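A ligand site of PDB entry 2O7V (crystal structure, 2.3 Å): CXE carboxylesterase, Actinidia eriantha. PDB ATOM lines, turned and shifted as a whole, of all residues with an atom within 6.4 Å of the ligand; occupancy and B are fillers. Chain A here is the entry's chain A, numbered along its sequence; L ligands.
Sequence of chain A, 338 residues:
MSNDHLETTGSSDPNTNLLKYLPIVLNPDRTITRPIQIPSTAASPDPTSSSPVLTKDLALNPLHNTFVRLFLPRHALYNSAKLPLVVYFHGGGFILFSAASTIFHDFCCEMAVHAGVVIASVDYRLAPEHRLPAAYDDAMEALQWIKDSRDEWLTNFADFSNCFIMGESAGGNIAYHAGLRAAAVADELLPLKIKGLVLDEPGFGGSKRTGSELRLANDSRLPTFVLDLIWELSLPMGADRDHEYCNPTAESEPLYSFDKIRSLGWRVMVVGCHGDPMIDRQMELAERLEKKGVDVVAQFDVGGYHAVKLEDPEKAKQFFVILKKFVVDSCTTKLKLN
Merely in contact with the ligand: His 306, Trp 231, Met 278, Leu 222, Ile 230, Gly 91 and Gly 203.
Within 4 Å of the ligand: Gly 91, Gly 92, Gly 93, Ser 169, Ala 170, Gly 203, Leu 222, Ile 230, Trp 231, Met 278 and His 306.
The side-chain hydroxyl of Ser 169 is covalently linked to a phosphorus (P1) of the ligand.
N of Gly 93 is in hydrogen-bond range of O3 of the ligand, 2.8 Å away.
N of Gly 92 lies within hydrogen-bond range of O3 of the ligand, at 2.9 Å.
N of Ala 170 is in hydrogen-bond range of O3 of the ligand (3.1 Å).
The side-chain hydroxyl of Ser 169 is in hydrogen-bond range of a ring nitrogen (NE2) of His 306, at 3.0 Å.
The backbone NH (N) of Gly 203 is in hydrogen-bond range of the backbone carbonyl oxygen (O) of Ser 169, at 2.7 Å.
N of Ser 169 sits close to O of Glu 201, 3.2 Å away.
NE2 of His 306 lies within hydrogen-bond range of OE2 of Glu 168, at 3.4 Å.
O of Glu 168 lies close to N of Gly 91 (3.3 Å).
The side-chain amide nitrogen (ND2) of Asn 173 sits at hydrogen-bond distance from the backbone carbonyl oxygen (O) of Gly 203, at 2.9 Å.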
ATOM      1  N   LEU A  22      -3.523  40.432 -16.415  1.00  0.00           N
ATOM      2  CA  LEU A  22      -4.714  39.716 -15.853  1.00  0.00           C
ATOM      3  C   LEU A  22      -5.433  40.638 -14.879  1.00  0.00           C
ATOM      4  O   LEU A  22      -4.793  41.351 -14.128  1.00  0.00           O
ATOM      5  CB  LEU A  22      -4.354  38.405 -15.145  1.00  0.00           C
ATOM      6  CG  LEU A  22      -3.642  37.338 -15.984  1.00  0.00           C
ATOM      7  CD1 LEU A  22      -2.724  36.521 -15.161  1.00  0.00           C
ATOM      8  CD2 LEU A  22      -4.587  36.455 -16.806  1.00  0.00           C
ATOM      9  N   HIS A  90     -15.380  27.830 -22.224  1.00  0.00           N
ATOM     10  CA  HIS A  90     -14.698  29.115 -22.393  1.00  0.00           C
ATOM     11  C   HIS A  90     -13.227  29.048 -21.958  1.00  0.00           C
ATOM     12  O   HIS A  90     -12.806  28.081 -21.294  1.00  0.00           O
ATOM     13  CB  HIS A  90     -15.483  30.279 -21.683  1.00  0.00           C
ATOM     14  CG  HIS A  90     -15.508  30.159 -20.192  1.00  0.00           C
ATOM     15  ND1 HIS A  90     -14.563  30.771 -19.377  1.00  0.00           N
ATOM     16  CD2 HIS A  90     -16.341  29.467 -19.357  1.00  0.00           C
ATOM     17  CE1 HIS A  90     -14.816  30.469 -18.117  1.00  0.00           C
ATOM     18  NE2 HIS A  90     -15.879  29.669 -18.070  1.00  0.00           N
ATOM     19  N   GLY A  91     -12.461  30.078 -22.339  1.00  0.00           N
ATOM     20  CA  GLY A  91     -11.039  30.227 -21.955  1.00  0.00           C
ATOM     21  C   GLY A  91     -10.938  31.176 -20.792  1.00  0.00           C
ATOM     22  O   GLY A  91     -11.940  31.620 -20.263  1.00  0.00           O
ATOM     23  N   GLY A  92      -9.713  31.510 -20.377  1.00  0.00           N
ATOM     24  CA  GLY A  92      -9.541  32.386 -19.208  1.00  0.00           C
ATOM     25  C   GLY A  92      -8.542  31.876 -18.187  1.00  0.00           C
ATOM     26  O   GLY A  92      -8.627  32.227 -17.030  1.00  0.00           O
ATOM     27  N   GLY A  93      -7.592  31.042 -18.585  1.00  0.00           N
ATOM     28  CA  GLY A  93      -6.617  30.497 -17.652  1.00  0.00           C
ATOM     29  C   GLY A  93      -7.087  29.641 -16.476  1.00  0.00           C
ATOM     30  O   GLY A  93      -6.315  29.410 -15.540  1.00  0.00           O
ATOM     31  N   PHE A  94      -8.333  29.172 -16.528  1.00  0.00           N
ATOM     32  CA  PHE A  94      -8.932  28.256 -15.546  1.00  0.00           C
ATOM     33  C   PHE A  94      -9.454  29.044 -14.349  1.00  0.00           C
ATOM     34  O   PHE A  94     -10.135  28.507 -13.482  1.00  0.00           O
ATOM     35  CB  PHE A  94      -7.980  27.184 -15.044  1.00  0.00           C
ATOM     36  CG  PHE A  94      -7.407  26.316 -16.119  1.00  0.00           C
ATOM     37  CD1 PHE A  94      -8.159  25.242 -16.645  1.00  0.00           C
ATOM     38  CD2 PHE A  94      -6.089  26.514 -16.583  1.00  0.00           C
ATOM     39  CE1 PHE A  94      -7.608  24.377 -17.619  1.00  0.00           C
ATOM     40  CE2 PHE A  94      -5.540  25.668 -17.572  1.00  0.00           C
ATOM     41  CZ  PHE A  94      -6.327  24.592 -18.088  1.00  0.00           C
ATOM     42  N   PHE A  97     -13.425  34.269 -16.155  1.00  0.00           N
ATOM     43  CA  PHE A  97     -14.544  34.257 -17.148  1.00  0.00           C
ATOM     44  C   PHE A  97     -15.689  33.292 -16.831  1.00  0.00           C
ATOM     45  O   PHE A  97     -15.639  32.520 -15.863  1.00  0.00           O
ATOM     46  CB  PHE A  97     -14.073  34.064 -18.615  1.00  0.00           C
ATOM     47  CG  PHE A  97     -13.220  35.215 -19.143  1.00  0.00           C
ATOM     48  CD1 PHE A  97     -13.793  36.236 -19.871  1.00  0.00           C
ATOM     49  CD2 PHE A  97     -11.819  35.245 -18.885  1.00  0.00           C
ATOM     50  CE1 PHE A  97     -12.961  37.317 -20.366  1.00  0.00           C
ATOM     51  CE2 PHE A  97     -11.031  36.293 -19.340  1.00  0.00           C
ATOM     52  CZ  PHE A  97     -11.599  37.345 -20.078  1.00  0.00           C
ATOM     53  N   GLU A 168     -12.058  26.897 -26.038  1.00  0.00           N
ATOM     54  CA  GLU A 168     -11.004  27.855 -26.341  1.00  0.00           C
ATOM     55  C   GLU A 168     -10.003  27.955 -25.197  1.00  0.00           C
ATOM     56  O   GLU A 168     -10.381  28.161 -24.035  1.00  0.00           O
ATOM     57  CB  GLU A 168     -11.604  29.237 -26.634  1.00  0.00           C
ATOM     58  CG  GLU A 168     -10.596  30.251 -27.136  1.00  0.00           C
ATOM     59  CD  GLU A 168      -9.974  31.062 -26.013  1.00  0.00           C
ATOM     60  OE1 GLU A 168     -10.571  31.106 -24.913  1.00  0.00           O
ATOM     61  OE2 GLU A 168      -8.899  31.654 -26.227  1.00  0.00           O
ATOM     62  N   SER A 169      -8.725  27.805 -25.518  1.00  0.00           N
ATOM     63  CA  SER A 169      -7.653  28.023 -24.548  1.00  0.00           C
ATOM     64  C   SER A 169      -7.707  26.977 -23.437  1.00  0.00           C
ATOM     65  O   SER A 169      -7.585  25.779 -23.692  1.00  0.00           O
ATOM     66  CB  SER A 169      -7.748  29.430 -23.958  1.00  0.00           C
ATOM     67  OG  SER A 169      -6.457  29.926 -23.627  1.00  0.00           O
ATOM     68  N   ALA A 170      -7.889  27.445 -22.202  1.00  0.00           N
ATOM     69  CA  ALA A 170      -8.081  26.550 -21.063  1.00  0.00           C
ATOM     70  C   ALA A 170      -9.288  25.644 -21.278  1.00  0.00           C
ATOM     71  O   ALA A 170      -9.235  24.447 -20.982  1.00  0.00           O
ATOM     72  CB  ALA A 170      -8.236  27.353 -19.784  1.00  0.00           C
ATOM     73  N   GLY A 171     -10.371  26.222 -21.787  1.00  0.00           N
ATOM     74  CA  GLY A 171     -11.533  25.418 -22.252  1.00  0.00           C
ATOM     75  C   GLY A 171     -11.223  24.398 -23.309  1.00  0.00           C
ATOM     76  O   GLY A 171     -11.887  23.405 -23.369  1.00  0.00           O
ATOM     77  N   ASN A 173      -8.083  23.003 -23.319  1.00  0.00           N
ATOM     78  CA  ASN A 173      -7.528  22.041 -22.365  1.00  0.00           C
ATOM     79  C   ASN A 173      -8.623  21.135 -21.764  1.00  0.00           C
ATOM     80  O   ASN A 173      -8.557  19.917 -21.922  1.00  0.00           O
ATOM     81  CB  ASN A 173      -6.690  22.719 -21.256  1.00  0.00           C
ATOM     82  CG  ASN A 173      -5.953  21.691 -20.317  1.00  0.00           C
ATOM     83  OD1 ASN A 173      -6.572  20.805 -19.698  1.00  0.00           O
ATOM     84  ND2 ASN A 173      -4.628  21.849 -20.190  1.00  0.00           N
ATOM     85  N   GLU A 201      -6.947  26.802 -29.954  1.00  0.00           N
ATOM     86  CA  GLU A 201      -5.743  27.189 -29.250  1.00  0.00           C
ATOM     87  C   GLU A 201      -5.769  26.642 -27.863  1.00  0.00           C
ATOM     88  O   GLU A 201      -5.823  27.439 -26.881  1.00  0.00           O
ATOM     89  CB  GLU A 201      -5.547  28.696 -29.174  1.00  0.00           C
ATOM     90  CG  GLU A 201      -6.208  29.515 -30.198  1.00  0.00           C
ATOM     91  CD  GLU A 201      -6.453  30.935 -29.713  1.00  0.00           C
ATOM     92  OE1 GLU A 201      -5.917  31.841 -30.378  1.00  0.00           O
ATOM     93  OE2 GLU A 201      -7.168  31.136 -28.686  1.00  0.00           O
ATOM     94  N   PRO A 202      -5.711  25.295 -27.766  1.00  0.00           N
ATOM     95  CA  PRO A 202      -5.929  24.709 -26.443  1.00  0.00           C
ATOM     96  C   PRO A 202      -4.729  25.124 -25.555  1.00  0.00           C
ATOM     97  O   PRO A 202      -3.621  25.312 -26.083  1.00  0.00           O
ATOM     98  CB  PRO A 202      -5.970  23.194 -26.741  1.00  0.00           C
ATOM     99  CG  PRO A 202      -5.165  23.036 -28.061  1.00  0.00           C
ATOM    100  CD  PRO A 202      -5.375  24.308 -28.812  1.00  0.00           C
ATOM    101  N   GLY A 203      -4.958  25.339 -24.261  1.00  0.00           N
ATOM    102  CA  GLY A 203      -3.916  25.851 -23.390  1.00  0.00           C
ATOM    103  C   GLY A 203      -3.098  24.769 -22.673  1.00  0.00           C
ATOM    104  O   GLY A 203      -3.612  23.992 -21.854  1.00  0.00           O
ATOM    105  N   PHE A 204      -1.786  24.754 -22.961  1.00  0.00           N
ATOM    106  CA  PHE A 204      -0.912  23.650 -22.595  1.00  0.00           C
ATOM    107  C   PHE A 204       0.421  24.139 -22.068  1.00  0.00           C
ATOM    108  O   PHE A 204       0.815  25.241 -22.401  1.00  0.00           O
ATOM    109  CB  PHE A 204      -0.694  22.745 -23.809  1.00  0.00           C
ATOM    110  CG  PHE A 204      -1.874  21.878 -24.105  1.00  0.00           C
ATOM    111  CD1 PHE A 204      -2.439  21.086 -23.104  1.00  0.00           C
ATOM    112  CD2 PHE A 204      -2.449  21.868 -25.367  1.00  0.00           C
ATOM    113  CE1 PHE A 204      -3.551  20.297 -23.353  1.00  0.00           C
ATOM    114  CE2 PHE A 204      -3.572  21.098 -25.637  1.00  0.00           C
ATOM    115  CZ  PHE A 204      -4.139  20.325 -24.651  1.00  0.00           C
ATOM    116  N   LEU A 222       0.279  37.218 -23.308  1.00  0.00           N
ATOM    117  CA  LEU A 222       0.724  36.037 -22.548  1.00  0.00           C
ATOM    118  C   LEU A 222       2.263  35.899 -22.255  1.00  0.00           C
ATOM    119  O   LEU A 222       2.911  34.918 -22.669  1.00  0.00           O
ATOM    120  CB  LEU A 222       0.149  34.771 -23.202  1.00  0.00           C
ATOM    121  CG  LEU A 222      -1.387  34.586 -23.116  1.00  0.00           C
ATOM    122  CD1 LEU A 222      -1.801  33.200 -23.632  1.00  0.00           C
ATOM    123  CD2 LEU A 222      -1.905  34.814 -21.676  1.00  0.00           C
ATOM    124  N   LEU A 227       1.792  33.128 -17.498  1.00  0.00           N
ATOM    125  CA  LEU A 227       1.492  31.705 -17.742  1.00  0.00           C
ATOM    126  C   LEU A 227       1.993  30.784 -16.688  1.00  0.00           C
ATOM    127  O   LEU A 227       1.327  29.821 -16.324  1.00  0.00           O
ATOM    128  CB  LEU A 227       2.060  31.274 -19.103  1.00  0.00           C
ATOM    129  CG  LEU A 227       1.351  31.877 -20.347  1.00  0.00           C
ATOM    130  CD1 LEU A 227       2.127  31.599 -21.601  1.00  0.00           C
ATOM    131  CD2 LEU A 227      -0.052  31.361 -20.471  1.00  0.00           C
ATOM    132  N   ILE A 230      -0.684  31.361 -14.059  1.00  0.00           N
ATOM    133  CA  ILE A 230      -1.861  30.540 -14.458  1.00  0.00           C
ATOM    134  C   ILE A 230      -1.715  29.096 -14.020  1.00  0.00           C
ATOM    135  O   ILE A 230      -2.548  28.591 -13.273  1.00  0.00           O
ATOM    136  CB  ILE A 230      -2.135  30.681 -16.023  1.00  0.00           C
ATOM    137  CG1 ILE A 230      -2.740  32.054 -16.294  1.00  0.00           C
ATOM    138  CG2 ILE A 230      -2.940  29.510 -16.611  1.00  0.00           C
ATOM    139  CD1 ILE A 230      -2.636  32.523 -17.773  1.00  0.00           C
ATOM    140  N   TRP A 231      -0.666  28.430 -14.448  1.00  0.00           N
ATOM    141  CA  TRP A 231      -0.448  27.021 -14.051  1.00  0.00           C
ATOM    142  C   TRP A 231      -0.214  26.792 -12.550  1.00  0.00           C
ATOM    143  O   TRP A 231      -0.438  25.694 -12.029  1.00  0.00           O
ATOM    144  CB  TRP A 231       0.726  26.437 -14.846  1.00  0.00           C
ATOM    145  CG  TRP A 231       0.393  26.290 -16.258  1.00  0.00           C
ATOM    146  CD1 TRP A 231       0.965  26.950 -17.309  1.00  0.00           C
ATOM    147  CD2 TRP A 231      -0.676  25.500 -16.814  1.00  0.00           C
ATOM    148  NE1 TRP A 231       0.360  26.590 -18.486  1.00  0.00           N
ATOM    149  CE2 TRP A 231      -0.645  25.705 -18.218  1.00  0.00           C
ATOM    150  CE3 TRP A 231      -1.634  24.613 -16.265  1.00  0.00           C
ATOM    151  CZ2 TRP A 231      -1.541  25.065 -19.084  1.00  0.00           C
ATOM    152  CZ3 TRP A 231      -2.523  23.973 -17.139  1.00  0.00           C
ATOM    153  CH2 TRP A 231      -2.464  24.192 -18.517  1.00  0.00           C
ATOM    154  N   MET A 278       1.881  29.358 -26.949  1.00  0.00           N
ATOM    155  CA  MET A 278       1.434  28.014 -26.749  1.00  0.00           C
ATOM    156  C   MET A 278       1.484  27.213 -28.014  1.00  0.00           C
ATOM    157  O   MET A 278       1.257  26.000 -27.976  1.00  0.00           O
ATOM    158  CB  MET A 278       0.076  27.974 -26.064  1.00  0.00           C
ATOM    159  CG  MET A 278       0.098  28.686 -24.685  1.00  0.00           C
ATOM    160  SD  MET A 278      -1.431  28.471 -23.796  1.00  0.00           S
ATOM    161  CE  MET A 278      -2.420  29.751 -24.484  1.00  0.00           C
ATOM    162  N   HIS A 306      -2.895  35.329 -29.574  1.00  0.00           N
ATOM    163  CA  HIS A 306      -3.796  34.479 -28.776  1.00  0.00           C
ATOM    164  C   HIS A 306      -5.146  35.127 -28.626  1.00  0.00           C
ATOM    165  O   HIS A 306      -5.225  36.248 -28.150  1.00  0.00           O
ATOM    166  CB  HIS A 306      -3.220  34.143 -27.389  1.00  0.00           C
ATOM    167  CG  HIS A 306      -4.065  33.164 -26.651  1.00  0.00           C
ATOM    168  ND1 HIS A 306      -3.939  31.799 -26.840  1.00  0.00           N
ATOM    169  CD2 HIS A 306      -5.141  33.333 -25.861  1.00  0.00           C
ATOM    170  CE1 HIS A 306      -4.865  31.173 -26.137  1.00  0.00           C
ATOM    171  NE2 HIS A 306      -5.616  32.084 -25.536  1.00  0.00           N
ATOM    172  N   ALA A 307      -6.208  34.433 -29.067  1.00  0.00           N
ATOM    173  CA  ALA A 307      -7.613  34.886 -28.903  1.00  0.00           C
ATOM    174  C   ALA A 307      -8.004  36.001 -29.883  1.00  0.00           C
ATOM    175  O   ALA A 307      -9.005  36.690 -29.679  1.00  0.00           O
ATOM    176  CB  ALA A 307      -7.915  35.294 -27.431  1.00  0.00           C
HETATM  177  C1  LIG L   1      -3.892  29.411 -20.491  1.00  0.00           C
HETATM  178  C2  LIG L   1      -3.435  28.000 -20.138  1.00  0.00           C
HETATM  179  C3  LIG L   1      -5.227  32.878 -21.055  1.00  0.00           C
HETATM  180  C4  LIG L   1      -5.556  34.205 -21.710  1.00  0.00           C
HETATM  181  O1  LIG L   1      -4.698  29.336 -21.663  1.00  0.00           O
HETATM  182  O2  LIG L   1      -5.008  31.824 -22.020  1.00  0.00           O
HETATM  183  O3  LIG L   1      -7.159  30.337 -21.214  1.00  0.00           O
HETATM  184  P1  LIG L   1      -5.793  30.421 -22.050  1.00  0.00           P
